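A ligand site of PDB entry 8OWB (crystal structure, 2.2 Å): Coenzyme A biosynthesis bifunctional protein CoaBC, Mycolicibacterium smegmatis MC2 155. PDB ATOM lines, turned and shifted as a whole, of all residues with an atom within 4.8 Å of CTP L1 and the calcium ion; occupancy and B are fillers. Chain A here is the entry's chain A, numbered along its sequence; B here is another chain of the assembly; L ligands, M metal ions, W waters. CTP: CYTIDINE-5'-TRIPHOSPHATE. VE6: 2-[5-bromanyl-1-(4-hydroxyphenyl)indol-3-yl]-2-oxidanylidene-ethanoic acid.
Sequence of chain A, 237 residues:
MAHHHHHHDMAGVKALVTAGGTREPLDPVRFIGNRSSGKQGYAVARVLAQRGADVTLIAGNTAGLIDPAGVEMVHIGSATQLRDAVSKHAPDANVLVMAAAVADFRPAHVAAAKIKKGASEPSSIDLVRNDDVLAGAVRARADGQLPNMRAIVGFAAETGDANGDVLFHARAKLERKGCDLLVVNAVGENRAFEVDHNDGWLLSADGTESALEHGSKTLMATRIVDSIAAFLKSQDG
An oxygen (O5') of CTP L1 lies within hydrogen-bond range of an oxygen (O17) of VE6 L2 (3.1 Å).
N of Asn 130 is in hydrogen-bond range of O of Asp 104 (2.9 Å). The side-chain carboxylate (OD1) of Asp 132 lies within hydrogen-bond range of the backbone NH (N) of Leu 134. The side-chain carboxylate of Glu 158 is in salt-bridge range of the side-chain amino group of Lys 173, at 2.5 Å. The side-chain amino group (NZ) of Lys 177 lies within salt-bridge range of the side-chain carboxylate (OD2) of Asp 132. The backbone carbonyl oxygen (O) of Ala 103 sits at hydrogen-bond distance from the side-chain amide nitrogen (ND2) of Asn 130 (3.0 Å).
The nearest printed residue that does not touch the calcium ion is Val 102 (4.8 Å).
Water W3 lies within hydrogen-bond range of the backbone carbonyl oxygen of Lys 117 of chain B and an oxygen (O2G) of CTP L1.
An oxygen (O3') of CTP L1 sits at hydrogen-bond distance from the backbone carbonyl oxygen (O) of Met 98, at 2.6 Å. The backbone NH of Leu 134 lies within hydrogen-bond range of an oxygen (O2) of CTP L1 (2.7 Å). O of Ala 100 lies within hydrogen-bond range of O2' of CTP L1. The backbone carbonyl oxygen (O) of Asp 131 lies within hydrogen-bond range of a nitrogen (N4) of CTP L1 (2.8 Å). An oxygen (O1A) of CTP L1 is in salt-bridge range of the side-chain amino group (NZ) of Lys 173 (2.9 Å). The backbone NH of Phe 155 sits at hydrogen-bond distance from an oxygen (O3') of CTP L1, at 3.0 Å. O of Phe 155 lies close to O3' of CTP L1 (3.3 Å). A nitrogen (N3) of CTP L1 lies within hydrogen-bond range of the backbone NH of Val 133 (3.2 Å). NZ of Lys 116 of chain B is in salt-bridge range of O1G of CTP L1 (3.9 Å). The backbone NH (N) of Lys 117 of chain B is in hydrogen-bond range of an oxygen (O2G) of CTP L1, 3.3 Å away. O1B of CTP L1 lies within salt-bridge range of NZ of Lys 177, at 3.9 Å.
Val 102 touches CTP L1 (CG1 to C4, 3.6 Å). Ala 103 touches CTP L1 (O to N4, 3.8 Å). OD1 of Asp 132 touches O2 of CTP L1, 3.5 Å away. Gly 154 touches CTP L1 (CA to O3', 3.9 Å). Hydrophobic or aromatic side chains that line CTP L1: Met 98, Val 102, Val 133, Leu 134 and Phe 155. Of the 20 residues printed, 15 come within 4 Å of CTP L1. Along chain A the residues within 4 Å of CTP L1 span positions 98 to 177.
The calcium ion is bound by O2B of CTP L1 (2.2 Å), OD2 of Asp 104 (2.3 Å), O2A of CTP L1 (2.5 Å), O3G of CTP L1 (2.5 Å), OD1 of Asp 104 (2.5 Å) and water W2 (2.9 Å). The calcium ion has six donor atoms within binding distance.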
ATOM      1  N   MET A  98     -17.412  -5.743  -3.472  1.00  0.00           N
ATOM      2  CA  MET A  98     -18.488  -6.114  -4.368  1.00  0.00           C
ATOM      3  C   MET A  98     -19.211  -4.863  -4.819  1.00  0.00           C
ATOM      4  O   MET A  98     -20.313  -4.554  -4.367  1.00  0.00           O
ATOM      5  CB  MET A  98     -19.441  -7.099  -3.679  1.00  0.00           C
ATOM      6  CG  MET A  98     -18.881  -8.500  -3.591  1.00  0.00           C
ATOM      7  SD  MET A  98     -18.719  -9.364  -5.170  1.00  0.00           S
ATOM      8  CE  MET A  98     -20.398  -9.506  -5.772  1.00  0.00           C
ATOM      9  N   ALA A  99     -18.618  -4.144  -5.766  1.00  0.00           N
ATOM     10  CA  ALA A  99     -19.241  -2.906  -6.212  1.00  0.00           C
ATOM     11  C   ALA A  99     -20.118  -3.072  -7.458  1.00  0.00           C
ATOM     12  O   ALA A  99     -20.614  -2.069  -7.971  1.00  0.00           O
ATOM     13  CB  ALA A  99     -18.172  -1.842  -6.483  1.00  0.00           C
ATOM     14  N   ALA A 100     -20.282  -4.292  -7.963  1.00  0.00           N
ATOM     15  CA  ALA A 100     -21.088  -4.525  -9.149  1.00  0.00           C
ATOM     16  C   ALA A 100     -22.570  -4.520  -8.818  1.00  0.00           C
ATOM     17  O   ALA A 100     -22.998  -4.988  -7.762  1.00  0.00           O
ATOM     18  CB  ALA A 100     -20.727  -5.849  -9.807  1.00  0.00           C
ATOM     19  N   VAL A 102     -25.162  -6.471  -9.331  1.00  0.00           N
ATOM     20  CA  VAL A 102     -25.469  -7.832  -9.741  1.00  0.00           C
ATOM     21  C   VAL A 102     -26.972  -7.987  -9.858  1.00  0.00           C
ATOM     22  O   VAL A 102     -27.710  -7.669  -8.915  1.00  0.00           O
ATOM     23  CB  VAL A 102     -24.866  -8.856  -8.756  1.00  0.00           C
ATOM     24  CG1 VAL A 102     -25.051 -10.256  -9.299  1.00  0.00           C
ATOM     25  CG2 VAL A 102     -23.376  -8.563  -8.506  1.00  0.00           C
ATOM     26  N   ALA A 103     -27.427  -8.485 -11.011  1.00  0.00           N
ATOM     27  CA  ALA A 103     -28.851  -8.667 -11.279  1.00  0.00           C
ATOM     28  C   ALA A 103     -29.461  -9.681 -10.328  1.00  0.00           C
ATOM     29  O   ALA A 103     -28.837 -10.711 -10.046  1.00  0.00           O
ATOM     30  CB  ALA A 103     -29.057  -9.119 -12.720  1.00  0.00           C
ATOM     31  N   ASP A 104     -30.645  -9.385  -9.795  1.00  0.00           N
ATOM     32  CA  ASP A 104     -31.262 -10.322  -8.861  1.00  0.00           C
ATOM     33  C   ASP A 104     -31.869 -11.550  -9.549  1.00  0.00           C
ATOM     34  O   ASP A 104     -31.910 -12.631  -8.949  1.00  0.00           O
ATOM     35  CB  ASP A 104     -32.332  -9.613  -8.010  1.00  0.00           C
ATOM     36  CG  ASP A 104     -31.748  -8.544  -7.080  1.00  0.00           C
ATOM     37  OD1 ASP A 104     -30.686  -8.776  -6.464  1.00  0.00           O
ATOM     38  OD2 ASP A 104     -32.369  -7.474  -6.926  1.00  0.00           O
ATOM     39  N   ASN A 130     -30.980 -15.316  -9.211  1.00  0.00           N
ATOM     40  CA  ASN A 130     -29.534 -15.441  -9.254  1.00  0.00           C
ATOM     41  C   ASN A 130     -28.972 -15.621  -7.849  1.00  0.00           C
ATOM     42  O   ASN A 130     -29.605 -15.261  -6.855  1.00  0.00           O
ATOM     43  CB  ASN A 130     -28.905 -14.209  -9.912  1.00  0.00           C
ATOM     44  CG  ASN A 130     -29.047 -14.210 -11.412  1.00  0.00           C
ATOM     45  OD1 ASN A 130     -29.116 -15.255 -12.038  1.00  0.00           O
ATOM     46  ND2 ASN A 130     -29.069 -13.033 -12.002  1.00  0.00           N
ATOM     47  N   ASP A 131     -27.792 -16.220  -7.769  1.00  0.00           N
ATOM     48  CA  ASP A 131     -27.154 -16.394  -6.477  1.00  0.00           C
ATOM     49  C   ASP A 131     -26.672 -15.057  -5.919  1.00  0.00           C
ATOM     50  O   ASP A 131     -26.326 -14.140  -6.657  1.00  0.00           O
ATOM     51  CB  ASP A 131     -25.957 -17.330  -6.583  1.00  0.00           C
ATOM     52  CG  ASP A 131     -26.356 -18.747  -6.823  1.00  0.00           C
ATOM     53  OD1 ASP A 131     -27.354 -19.210  -6.226  1.00  0.00           O
ATOM     54  OD2 ASP A 131     -25.630 -19.421  -7.585  1.00  0.00           O
ATOM     55  N   ASP A 132     -26.729 -14.937  -4.596  1.00  0.00           N
ATOM     56  CA  ASP A 132     -26.165 -13.790  -3.893  1.00  0.00           C
ATOM     57  C   ASP A 132     -24.680 -14.056  -3.687  1.00  0.00           C
ATOM     58  O   ASP A 132     -24.276 -14.838  -2.815  1.00  0.00           O
ATOM     59  CB  ASP A 132     -26.877 -13.561  -2.569  1.00  0.00           C
ATOM     60  CG  ASP A 132     -26.418 -12.315  -1.877  1.00  0.00           C
ATOM     61  OD1 ASP A 132     -25.330 -11.818  -2.220  1.00  0.00           O
ATOM     62  OD2 ASP A 132     -27.130 -11.830  -0.972  1.00  0.00           O
ATOM     63  N   VAL A 133     -23.850 -13.393  -4.492  1.00  0.00           N
ATOM     64  CA  VAL A 133     -22.410 -13.639  -4.436  1.00  0.00           C
ATOM     65  C   VAL A 133     -21.793 -13.004  -3.198  1.00  0.00           C
ATOM     66  O   VAL A 133     -20.895 -13.581  -2.563  1.00  0.00           O
ATOM     67  CB  VAL A 133     -21.751 -13.152  -5.734  1.00  0.00           C
ATOM     68  CG1 VAL A 133     -20.315 -13.609  -5.789  1.00  0.00           C
ATOM     69  CG2 VAL A 133     -22.515 -13.677  -6.942  1.00  0.00           C
ATOM     70  N   LEU A 134     -22.237 -11.802  -2.825  1.00  0.00           N
ATOM     71  CA  LEU A 134     -21.697 -11.197  -1.607  1.00  0.00           C
ATOM     72  C   LEU A 134     -22.009 -12.061  -0.396  1.00  0.00           C
ATOM     73  O   LEU A 134     -21.122 -12.282   0.448  1.00  0.00           O
ATOM     74  CB  LEU A 134     -22.221  -9.771  -1.429  1.00  0.00           C
ATOM     75  CG  LEU A 134     -21.764  -9.031  -0.165  1.00  0.00           C
ATOM     76  CD1 LEU A 134     -20.271  -8.821  -0.160  1.00  0.00           C
ATOM     77  CD2 LEU A 134     -22.506  -7.715   0.015  1.00  0.00           C
ATOM     78  N   GLY A 154     -19.324  -4.695   0.813  1.00  0.00           N
ATOM     79  CA  GLY A 154     -20.470  -4.613  -0.051  1.00  0.00           C
ATOM     80  C   GLY A 154     -20.847  -3.168  -0.371  1.00  0.00           C
ATOM     81  O   GLY A 154     -20.371  -2.223   0.255  1.00  0.00           O
ATOM     82  N   PHE A 155     -21.681  -3.018  -1.397  1.00  0.00           N
ATOM     83  CA  PHE A 155     -22.136  -1.706  -1.848  1.00  0.00           C
ATOM     84  C   PHE A 155     -23.649  -1.691  -1.883  1.00  0.00           C
ATOM     85  O   PHE A 155     -24.277  -2.716  -2.081  1.00  0.00           O
ATOM     86  CB  PHE A 155     -21.612  -1.381  -3.226  1.00  0.00           C
ATOM     87  CG  PHE A 155     -20.279  -0.729  -3.213  1.00  0.00           C
ATOM     88  CD1 PHE A 155     -19.214  -1.314  -2.546  1.00  0.00           C
ATOM     89  CD2 PHE A 155     -20.064   0.445  -3.894  1.00  0.00           C
ATOM     90  CE1 PHE A 155     -17.976  -0.721  -2.543  1.00  0.00           C
ATOM     91  CE2 PHE A 155     -18.813   1.036  -3.911  1.00  0.00           C
ATOM     92  CZ  PHE A 155     -17.769   0.462  -3.229  1.00  0.00           C
ATOM     93  N   ALA A 156     -24.224  -0.526  -1.614  1.00  0.00           N
ATOM     94  CA  ALA A 156     -25.671  -0.401  -1.668  1.00  0.00           C
ATOM     95  C   ALA A 156     -26.049   1.052  -1.927  1.00  0.00           C
ATOM     96  O   ALA A 156     -25.347   1.990  -1.527  1.00  0.00           O
ATOM     97  CB  ALA A 156     -26.321  -0.916  -0.377  1.00  0.00           C
ATOM     98  N   GLU A 158     -29.397   3.173  -1.083  1.00  0.00           N
ATOM     99  CA  GLU A 158     -30.617   3.057  -0.291  1.00  0.00           C
ATOM    100  C   GLU A 158     -31.357   4.389  -0.270  1.00  0.00           C
ATOM    101  O   GLU A 158     -30.755   5.463  -0.368  1.00  0.00           O
ATOM    102  CB  GLU A 158     -30.317   2.606   1.153  1.00  0.00           C
ATOM    103  CG  GLU A 158     -29.666   1.227   1.312  1.00  0.00           C
ATOM    104  CD  GLU A 158     -30.589   0.085   0.902  1.00  0.00           C
ATOM    105  OE1 GLU A 158     -31.823   0.210   1.090  1.00  0.00           O
ATOM    106  OE2 GLU A 158     -30.066  -0.937   0.405  1.00  0.00           O
ATOM    107  N   LYS A 173     -29.445  -3.638   5.760  1.00  0.00           N
ATOM    108  CA  LYS A 173     -28.662  -4.271   4.707  1.00  0.00           C
ATOM    109  C   LYS A 173     -27.358  -4.830   5.248  1.00  0.00           C
ATOM    110  O   LYS A 173     -27.001  -5.984   4.970  1.00  0.00           O
ATOM    111  CB  LYS A 173     -28.368  -3.229   3.632  1.00  0.00           C
ATOM    112  CG  LYS A 173     -29.255  -3.297   2.456  1.00  0.00           C
ATOM    113  CD  LYS A 173     -28.847  -4.411   1.551  1.00  0.00           C
ATOM    114  CE  LYS A 173     -29.929  -4.603   0.518  1.00  0.00           C
ATOM    115  NZ  LYS A 173     -30.157  -3.361  -0.258  1.00  0.00           N
ATOM    116  N   LYS A 177     -26.507  -8.671   5.211  1.00  0.00           N
ATOM    117  CA  LYS A 177     -25.427  -9.152   4.358  1.00  0.00           C
ATOM    118  C   LYS A 177     -24.294  -9.729   5.172  1.00  0.00           C
ATOM    119  O   LYS A 177     -23.654 -10.703   4.766  1.00  0.00           O
ATOM    120  CB  LYS A 177     -24.907  -8.019   3.470  1.00  0.00           C
ATOM    121  CG  LYS A 177     -25.870  -7.629   2.342  1.00  0.00           C
ATOM    122  CD  LYS A 177     -26.156  -8.805   1.437  1.00  0.00           C
ATOM    123  CE  LYS A 177     -27.013  -8.385   0.274  1.00  0.00           C
ATOM    124  NZ  LYS A 177     -26.817  -9.311  -0.893  1.00  0.00           N
ATOM    125  N   ILE B 115     -37.598  -2.776  -7.656  1.00  0.00           N
ATOM    126  CA  ILE B 115     -38.308  -3.929  -7.123  1.00  0.00           C
ATOM    127  C   ILE B 115     -37.366  -4.677  -6.194  1.00  0.00           C
ATOM    128  O   ILE B 115     -36.289  -5.130  -6.609  1.00  0.00           O
ATOM    129  CB  ILE B 115     -38.805  -4.814  -8.278  1.00  0.00           C
ATOM    130  CG1 ILE B 115     -39.330  -3.915  -9.403  1.00  0.00           C
ATOM    131  CG2 ILE B 115     -39.888  -5.765  -7.814  1.00  0.00           C
ATOM    132  CD1 ILE B 115     -39.744  -4.654 -10.660  1.00  0.00           C
ATOM    133  N   LYS B 116     -37.752  -4.808  -4.918  1.00  0.00           N
ATOM    134  CA  LYS B 116     -36.865  -5.487  -3.986  1.00  0.00           C
ATOM    135  C   LYS B 116     -36.890  -6.981  -4.277  1.00  0.00           C
ATOM    136  O   LYS B 116     -37.893  -7.530  -4.766  1.00  0.00           O
ATOM    137  CB  LYS B 116     -37.266  -5.227  -2.523  1.00  0.00           C
ATOM    138  CG  LYS B 116     -37.264  -3.764  -2.036  1.00  0.00           C
ATOM    139  CD  LYS B 116     -35.969  -3.025  -2.406  1.00  0.00           C
ATOM    140  CE  LYS B 116     -35.596  -1.873  -1.464  1.00  0.00           C
ATOM    141  NZ  LYS B 116     -35.719  -2.182   0.005  1.00  0.00           N
ATOM    142  N   LYS B 117     -35.756  -7.631  -4.033  1.00  0.00           N
ATOM    143  CA  LYS B 117     -35.673  -9.079  -4.190  1.00  0.00           C
ATOM    144  C   LYS B 117     -36.615  -9.752  -3.212  1.00  0.00           C
ATOM    145  O   LYS B 117     -36.600  -9.455  -2.006  1.00  0.00           O
ATOM    146  CB  LYS B 117     -34.235  -9.556  -3.968  1.00  0.00           C
HETATM  147  N1  CTP L   1     -24.965  -8.595  -4.922  1.00  0.00           N
HETATM  148  C2  CTP L   1     -24.467  -9.870  -5.092  1.00  0.00           C
HETATM  149  N3  CTP L   1     -25.211 -10.827  -5.742  1.00  0.00           N
HETATM  150  C4  CTP L   1     -26.531 -10.568  -6.072  1.00  0.00           C
HETATM  151  C5  CTP L   1     -27.082  -9.313  -5.745  1.00  0.00           C
HETATM  152  C6  CTP L   1     -26.306  -8.367  -5.093  1.00  0.00           C
HETATM  153  O2  CTP L   1     -23.353 -10.173  -4.658  1.00  0.00           O
HETATM  154  N4  CTP L   1     -27.245 -11.510  -6.705  1.00  0.00           N
HETATM  155  C1' CTP L   1     -24.177  -7.661  -4.108  1.00  0.00           C
HETATM  156  C2' CTP L   1     -23.908  -6.345  -4.822  1.00  0.00           C
HETATM  157  O2' CTP L   1     -22.666  -6.364  -5.462  1.00  0.00           O
HETATM  158  C3' CTP L   1     -23.879  -5.364  -3.686  1.00  0.00           C
HETATM  159  C4' CTP L   1     -24.638  -6.016  -2.553  1.00  0.00           C
HETATM  160  O4' CTP L   1     -24.886  -7.344  -2.931  1.00  0.00           O
HETATM  161  O3' CTP L   1     -22.551  -5.216  -3.256  1.00  0.00           O
HETATM  162  C5' CTP L   1     -25.992  -5.382  -2.273  1.00  0.00           C
HETATM  163  O5' CTP L   1     -26.753  -5.155  -3.444  1.00  0.00           O
HETATM  164  PA  CTP L   1     -28.316  -4.863  -3.210  1.00  0.00           P
HETATM  165  O1A CTP L   1     -28.487  -3.488  -2.619  1.00  0.00           O
HETATM  166  O2A CTP L   1     -29.129  -5.081  -4.475  1.00  0.00           O
HETATM  167  O3A CTP L   1     -28.631  -6.011  -2.123  1.00  0.00           O
HETATM  168  PB  CTP L   1     -30.018  -6.756  -2.318  1.00  0.00           P
HETATM  169  O1B CTP L   1     -30.373  -7.743  -1.237  1.00  0.00           O
HETATM  170  O2B CTP L   1     -30.119  -7.349  -3.701  1.00  0.00           O
HETATM  171  O3B CTP L   1     -30.915  -5.427  -2.263  1.00  0.00           O
HETATM  172  PG  CTP L   1     -32.471  -5.333  -2.654  1.00  0.00           P
HETATM  173  O1G CTP L   1     -32.965  -4.110  -1.919  1.00  0.00           O
HETATM  174  O2G CTP L   1     -33.203  -6.572  -2.193  1.00  0.00           O
HETATM  175  O3G CTP L   1     -32.564  -5.181  -4.148  1.00  0.00           O
HETATM  176  N12 VE6 L   2     -23.209   1.435  -6.403  1.00  0.00           N
HETATM  177  C13 VE6 L   2     -23.990   0.268  -6.234  1.00  0.00           C
HETATM  178  C15 VE6 L   2     -25.996  -0.831  -5.519  1.00  0.00           C
HETATM  179  C20 VE6 L   2     -22.779   2.272  -5.458  1.00  0.00           C
HETATM  180  C21 VE6 L   2     -22.940   2.301  -4.065  1.00  0.00           C
HETATM  181  C22 VE6 L   2     -22.361   3.326  -3.326  1.00  0.00           C
HETATM  182  C02 VE6 L   2     -21.623   4.338  -3.954  1.00  0.00           C
HETATM  183  C03 VE6 L   2     -21.470   4.324  -5.329  1.00  0.00           C
HETATM  184  C04 VE6 L   2     -22.046   3.289  -6.070  1.00  0.00           C
HETATM  185  C05 VE6 L   2     -22.060   2.997  -7.481  1.00  0.00           C
HETATM  186  C06 VE6 L   2     -21.385   3.815  -8.566  1.00  0.00           C
HETATM  187  C07 VE6 L   2     -20.588   3.221  -9.724  1.00  0.00           C
HETATM  188  C11 VE6 L   2     -22.802   1.823  -7.604  1.00  0.00           C
HETATM  189  C14 VE6 L   2     -25.262   0.327  -5.669  1.00  0.00           C
HETATM  190  C16 VE6 L   2     -25.475  -2.046  -5.922  1.00  0.00           C
HETATM  191  C18 VE6 L   2     -24.218  -2.112  -6.476  1.00  0.00           C
HETATM  192  C19 VE6 L   2     -23.477  -0.951  -6.631  1.00  0.00           C
HETATM  193  O08 VE6 L   2     -20.628   3.848 -10.834  1.00  0.00           O
HETATM  194  O09 VE6 L   2     -19.920   2.149  -9.619  1.00  0.00           O
HETATM  195  O10 VE6 L   2     -21.479   5.030  -8.526  1.00  0.00           O
HETATM  196  O17 VE6 L   2     -26.243  -3.215  -5.773  1.00  0.00           O
HETATM  197 BR01 VE6 L   2     -20.815   5.751  -2.915  1.00  0.00          BR
HETATM  198 CA    CA M   1     -30.900  -6.409  -5.583  1.00  0.00          CA
HETATM  199  O   HOH W   1     -29.922 -11.085  -6.158  1.00  0.00           O
HETATM  200  O   HOH W   2     -28.345  -6.349  -6.921  1.00  0.00           O
HETATM  201  O   HOH W   3     -35.982  -7.663  -0.492  1.00  0.00           O
